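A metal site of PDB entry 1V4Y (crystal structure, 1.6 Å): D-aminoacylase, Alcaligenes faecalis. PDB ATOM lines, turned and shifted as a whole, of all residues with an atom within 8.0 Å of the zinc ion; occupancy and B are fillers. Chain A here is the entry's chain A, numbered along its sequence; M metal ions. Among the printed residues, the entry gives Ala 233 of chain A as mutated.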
ATOM      1  N   HIS A  80       4.183   8.782   9.532  1.00  0.00           N
ATOM      2  CA  HIS A  80       3.378   9.638   8.669  1.00  0.00           C
ATOM      3  C   HIS A  80       2.537  10.645   9.441  1.00  0.00           C
ATOM      4  O   HIS A  80       1.439  10.321   9.896  1.00  0.00           O
ATOM      5  CB  HIS A  80       2.455   8.790   7.791  1.00  0.00           C
ATOM      6  CG  HIS A  80       1.773   9.560   6.699  1.00  0.00           C
ATOM      7  ND1 HIS A  80       2.249   9.581   5.404  1.00  0.00           N
ATOM      8  CD2 HIS A  80       0.670  10.339   6.718  1.00  0.00           C
ATOM      9  CE1 HIS A  80       1.458  10.342   4.668  1.00  0.00           C
ATOM     10  NE2 HIS A  80       0.496  10.813   5.440  1.00  0.00           N
ATOM     11  N   THR A  81       3.046  11.859   9.588  1.00  0.00           N
ATOM     12  CA  THR A  81       2.316  12.886  10.302  1.00  0.00           C
ATOM     13  C   THR A  81       2.163  14.157   9.490  1.00  0.00           C
ATOM     14  O   THR A  81       2.815  14.351   8.460  1.00  0.00           O
ATOM     15  CB  THR A  81       3.030  13.315  11.605  1.00  0.00           C
ATOM     16  OG1 THR A  81       4.062  14.259  11.305  1.00  0.00           O
ATOM     17  CG2 THR A  81       3.639  12.114  12.314  1.00  0.00           C
ATOM     18  N   HIS A  82       1.273  15.011   9.971  1.00  0.00           N
ATOM     19  CA  HIS A  82       1.033  16.326   9.397  1.00  0.00           C
ATOM     20  C   HIS A  82       1.126  17.260  10.590  1.00  0.00           C
ATOM     21  O   HIS A  82       0.278  18.136  10.788  1.00  0.00           O
ATOM     22  CB  HIS A  82      -0.351  16.372   8.743  1.00  0.00           C
ATOM     23  CG  HIS A  82      -0.432  15.558   7.500  1.00  0.00           C
ATOM     24  ND1 HIS A  82       0.307  15.841   6.377  1.00  0.00           N
ATOM     25  CD2 HIS A  82      -1.133  14.429   7.212  1.00  0.00           C
ATOM     26  CE1 HIS A  82       0.084  14.926   5.448  1.00  0.00           C
ATOM     27  NE2 HIS A  82      -0.793  14.059   5.931  1.00  0.00           N
ATOM     28  N   GLY A 107       5.866  16.728   6.928  1.00  0.00           N
ATOM     29  CA  GLY A 107       5.890  17.084   5.515  1.00  0.00           C
ATOM     30  C   GLY A 107       5.515  15.978   4.565  1.00  0.00           C
ATOM     31  O   GLY A 107       6.225  15.706   3.595  1.00  0.00           O
ATOM     32  N   ASN A 108       4.377  15.331   4.827  1.00  0.00           N
ATOM     33  CA  ASN A 108       3.918  14.220   3.995  1.00  0.00           C
ATOM     34  C   ASN A 108       2.863  14.568   2.951  1.00  0.00           C
ATOM     35  O   ASN A 108       2.253  15.638   2.998  1.00  0.00           O
ATOM     36  CB  ASN A 108       3.383  13.110   4.899  1.00  0.00           C
ATOM     37  CG  ASN A 108       4.484  12.438   5.692  1.00  0.00           C
ATOM     38  OD1 ASN A 108       4.726  12.754   6.863  1.00  0.00           O
ATOM     39  ND2 ASN A 108       5.187  11.519   5.047  1.00  0.00           N
ATOM     40  N   CYS A 109       2.668  13.652   2.000  1.00  0.00           N
ATOM     41  CA  CYS A 109       1.695  13.823   0.922  1.00  0.00           C
ATOM     42  C   CYS A 109       1.932  15.085   0.104  1.00  0.00           C
ATOM     43  O   CYS A 109       0.991  15.649  -0.457  1.00  0.00           O
ATOM     44  CB  CYS A 109       0.274  13.848   1.496  1.00  0.00           C
ATOM     45  SG  CYS A 109      -0.159  12.344   2.388  1.00  0.00           S
ATOM     46  N   GLY A 110       3.190  15.508   0.034  1.00  0.00           N
ATOM     47  CA  GLY A 110       3.542  16.694  -0.713  1.00  0.00           C
ATOM     48  C   GLY A 110       3.187  17.981   0.026  1.00  0.00           C
ATOM     49  O   GLY A 110       3.345  19.077  -0.512  1.00  0.00           O
ATOM     50  N   ILE A 111       2.725  17.830   1.265  1.00  0.00           N
ATOM     51  CA  ILE A 111       2.312  18.958   2.099  1.00  0.00           C
ATOM     52  C   ILE A 111       3.306  19.282   3.213  1.00  0.00           C
ATOM     53  O   ILE A 111       3.419  18.535   4.183  1.00  0.00           O
ATOM     54  CB  ILE A 111       0.954  18.651   2.787  1.00  0.00           C
ATOM     55  CG1 ILE A 111      -0.078  18.201   1.751  1.00  0.00           C
ATOM     56  CG2 ILE A 111       0.468  19.885   3.535  1.00  0.00           C
ATOM     57  CD1 ILE A 111      -1.351  17.653   2.371  1.00  0.00           C
ATOM     58  N   LEU A 127      -4.588  22.171   5.642  1.00  0.00           N
ATOM     59  CA  LEU A 127      -4.761  21.250   6.766  1.00  0.00           C
ATOM     60  C   LEU A 127      -3.754  21.564   7.873  1.00  0.00           C
ATOM     61  O   LEU A 127      -3.945  21.166   9.020  1.00  0.00           O
ATOM     62  CB  LEU A 127      -4.578  19.795   6.298  1.00  0.00           C
ATOM     63  CG  LEU A 127      -5.680  19.215   5.399  1.00  0.00           C
ATOM     64  CD1 LEU A 127      -5.278  17.827   4.914  1.00  0.00           C
ATOM     65  CD2 LEU A 127      -6.991  19.146   6.177  1.00  0.00           C
ATOM     66  N   TYR A 205      -3.908  15.135  -5.126  1.00  0.00           N
ATOM     67  CA  TYR A 205      -4.489  16.431  -4.792  1.00  0.00           C
ATOM     68  C   TYR A 205      -4.354  17.531  -5.861  1.00  0.00           C
ATOM     69  O   TYR A 205      -3.396  17.548  -6.637  1.00  0.00           O
ATOM     70  CB  TYR A 205      -3.922  16.886  -3.454  1.00  0.00           C
ATOM     71  CG  TYR A 205      -4.211  15.871  -2.369  1.00  0.00           C
ATOM     72  CD1 TYR A 205      -5.485  15.750  -1.835  1.00  0.00           C
ATOM     73  CD2 TYR A 205      -3.218  14.999  -1.919  1.00  0.00           C
ATOM     74  CE1 TYR A 205      -5.788  14.774  -0.893  1.00  0.00           C
ATOM     75  CE2 TYR A 205      -3.506  14.009  -0.971  1.00  0.00           C
ATOM     76  CZ  TYR A 205      -4.789  13.908  -0.459  1.00  0.00           C
ATOM     77  OH  TYR A 205      -5.085  12.939   0.468  1.00  0.00           O
ATOM     78  N   ALA A 233       2.060   9.947  -1.518  1.00  0.00           N
ATOM     79  CA  ALA A 233       0.656   9.601  -1.382  1.00  0.00           C
ATOM     80  C   ALA A 233       0.423   9.369  -2.879  1.00  0.00           C
ATOM     81  O   ALA A 233       0.362  10.313  -3.659  1.00  0.00           O
ATOM     82  CB  ALA A 233      -0.148  10.805  -0.893  1.00  0.00           C
ATOM     83  N   SER A 262       3.049   5.974   1.169  1.00  0.00           N
ATOM     84  CA  SER A 262       2.248   6.452   2.305  1.00  0.00           C
ATOM     85  C   SER A 262       0.842   5.879   2.388  1.00  0.00           C
ATOM     86  O   SER A 262       0.205   5.611   1.372  1.00  0.00           O
ATOM     87  CB  SER A 262       2.155   7.976   2.272  1.00  0.00           C
ATOM     88  OG  SER A 262       3.442   8.568   2.260  1.00  0.00           O
ATOM     89  N   HIS A 263       0.359   5.727   3.617  1.00  0.00           N
ATOM     90  CA  HIS A 263      -0.974   5.209   3.919  1.00  0.00           C
ATOM     91  C   HIS A 263      -1.503   4.234   2.871  1.00  0.00           C
ATOM     92  O   HIS A 263      -2.546   4.475   2.254  1.00  0.00           O
ATOM     93  CB  HIS A 263      -1.971   6.375   4.117  1.00  0.00           C
ATOM     94  CG  HIS A 263      -1.976   7.382   3.010  1.00  0.00           C
ATOM     95  ND1 HIS A 263      -2.228   7.060   1.696  1.00  0.00           N
ATOM     96  CD2 HIS A 263      -1.770   8.721   3.032  1.00  0.00           C
ATOM     97  CE1 HIS A 263      -2.186   8.155   0.958  1.00  0.00           C
ATOM     98  NE2 HIS A 263      -1.910   9.177   1.740  1.00  0.00           N
ATOM     99  N   ASP A 294       3.830   2.502   4.750  1.00  0.00           N
ATOM    100  CA  ASP A 294       3.263   2.605   6.075  1.00  0.00           C
ATOM    101  C   ASP A 294       1.754   2.650   5.942  1.00  0.00           C
ATOM    102  O   ASP A 294       1.225   2.748   4.835  1.00  0.00           O
ATOM    103  CB  ASP A 294       3.779   3.824   6.850  1.00  0.00           C
ATOM    104  CG  ASP A 294       3.427   5.153   6.192  1.00  0.00           C
ATOM    105  OD1 ASP A 294       2.290   5.330   5.723  1.00  0.00           O
ATOM    106  OD2 ASP A 294       4.312   6.041   6.183  1.00  0.00           O
ATOM    107  N   TYR A 296      -2.184   3.250   8.524  1.00  0.00           N
ATOM    108  CA  TYR A 296      -2.836   3.488   9.802  1.00  0.00           C
ATOM    109  C   TYR A 296      -3.890   2.387   9.971  1.00  0.00           C
ATOM    110  O   TYR A 296      -4.461   1.891   8.992  1.00  0.00           O
ATOM    111  CB  TYR A 296      -3.457   4.887   9.859  1.00  0.00           C
ATOM    112  CG  TYR A 296      -4.320   5.259   8.685  1.00  0.00           C
ATOM    113  CD1 TYR A 296      -5.638   4.808   8.603  1.00  0.00           C
ATOM    114  CD2 TYR A 296      -3.827   6.059   7.662  1.00  0.00           C
ATOM    115  CE1 TYR A 296      -6.450   5.160   7.517  1.00  0.00           C
ATOM    116  CE2 TYR A 296      -4.618   6.407   6.577  1.00  0.00           C
ATOM    117  CZ  TYR A 296      -5.923   5.960   6.515  1.00  0.00           C
ATOM    118  OH  TYR A 296      -6.710   6.300   5.435  1.00  0.00           O
ATOM    119  N   SER A 302      -8.916  10.392   5.905  1.00  0.00           N
ATOM    120  CA  SER A 302      -9.257  11.770   6.236  1.00  0.00           C
ATOM    121  C   SER A 302      -8.291  12.727   5.547  1.00  0.00           C
ATOM    122  O   SER A 302      -7.084  12.489   5.505  1.00  0.00           O
ATOM    123  CB  SER A 302      -9.217  11.993   7.753  1.00  0.00           C
ATOM    124  OG  SER A 302      -9.728  13.275   8.104  1.00  0.00           O
ATOM    125  N   THR A 303      -8.839  13.795   4.996  1.00  0.00           N
ATOM    126  CA  THR A 303      -8.055  14.807   4.306  1.00  0.00           C
ATOM    127  C   THR A 303      -8.992  15.947   3.930  1.00  0.00           C
ATOM    128  O   THR A 303     -10.047  16.118   4.543  1.00  0.00           O
ATOM    129  CB  THR A 303      -7.376  14.229   3.033  1.00  0.00           C
ATOM    130  OG1 THR A 303      -6.582  15.243   2.410  1.00  0.00           O
ATOM    131  CG2 THR A 303      -8.413  13.708   2.045  1.00  0.00           C
ATOM    132  N   SER A 378       0.286   7.417  11.756  1.00  0.00           N
ATOM    133  CA  SER A 378      -1.050   7.886  12.154  1.00  0.00           C
ATOM    134  C   SER A 378      -1.826   8.691  11.126  1.00  0.00           C
ATOM    135  O   SER A 378      -3.052   8.561  11.033  1.00  0.00           O
ATOM    136  CB  SER A 378      -0.940   8.726  13.429  1.00  0.00           C
ATOM    137  OG  SER A 378      -0.391  10.005  13.146  1.00  0.00           O
ATOM    138  N   ASP A 379      -1.121   9.521  10.363  1.00  0.00           N
ATOM    139  CA  ASP A 379      -1.743  10.394   9.363  1.00  0.00           C
ATOM    140  C   ASP A 379      -2.714  11.312  10.095  1.00  0.00           C
ATOM    141  O   ASP A 379      -3.732  11.734   9.540  1.00  0.00           O
ATOM    142  CB  ASP A 379      -2.474   9.574   8.296  1.00  0.00           C
ATOM    143  CG  ASP A 379      -2.643  10.333   6.995  1.00  0.00           C
ATOM    144  OD1 ASP A 379      -2.210  11.496   6.911  1.00  0.00           O
ATOM    145  OD2 ASP A 379      -3.210   9.758   6.045  1.00  0.00           O
ATOM    146  N   GLY A 380      -2.406  11.621  11.346  1.00  0.00           N
ATOM    147  CA  GLY A 380      -3.277  12.495  12.109  1.00  0.00           C
ATOM    148  C   GLY A 380      -3.298  13.919  11.575  1.00  0.00           C
ATOM    149  O   GLY A 380      -2.287  14.428  11.083  1.00  0.00           O
ATOM    150  N   LEU A 381      -4.462  14.557  11.634  1.00  0.00           N
ATOM    151  CA  LEU A 381      -4.636  15.935  11.184  1.00  0.00           C
ATOM    152  C   LEU A 381      -4.994  16.661  12.483  1.00  0.00           C
ATOM    153  O   LEU A 381      -6.166  16.827  12.821  1.00  0.00           O
ATOM    154  CB  LEU A 381      -5.782  16.000  10.153  1.00  0.00           C
ATOM    155  CG  LEU A 381      -5.514  15.106   8.931  1.00  0.00           C
ATOM    156  CD1 LEU A 381      -6.695  15.148   7.970  1.00  0.00           C
ATOM    157  CD2 LEU A 381      -4.253  15.572   8.230  1.00  0.00           C
ATOM    158  N   ARG A 390      -7.547   8.455  14.590  1.00  0.00           N
ATOM    159  CA  ARG A 390      -6.185   7.959  14.374  1.00  0.00           C
ATOM    160  C   ARG A 390      -5.184   8.941  14.978  1.00  0.00           C
ATOM    161  O   ARG A 390      -4.069   8.564  15.371  1.00  0.00           O
ATOM    162  CB  ARG A 390      -5.917   7.770  12.877  1.00  0.00           C
ATOM    163  CG  ARG A 390      -5.945   9.042  12.050  1.00  0.00           C
ATOM    164  CD  ARG A 390      -6.054   8.712  10.578  1.00  0.00           C
ATOM    165  NE  ARG A 390      -5.828   9.866   9.716  1.00  0.00           N
ATOM    166  CZ  ARG A 390      -6.052   9.875   8.410  1.00  0.00           C
ATOM    167  NH1 ARG A 390      -6.502   8.787   7.802  1.00  0.00           N
ATOM    168  NH2 ARG A 390      -5.794  10.962   7.694  1.00  0.00           N
HETATM  169 ZN    ZN M   1      -0.938  12.244   5.050  1.00  0.00          ZN
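The guanidinium group of Arg 390 lies within salt-bridge range of the side-chain carboxylate of Asp 379.
SG of Cys 109 sits close to NE2 of His 263, 3.7 Å away.
The zinc ion is bound by NE2 of His 82 (2.0 Å), NE2 of His 80 (2.1 Å), OD1 of Asp 379 (2.4 Å) and SG of Cys 109 (2.8 Å).
The zinc ion has four donor atoms within binding distance.
Four residues have an atom within 4 Å of the zinc ion: His 80, His 82, Cys 109 and Asp 379.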
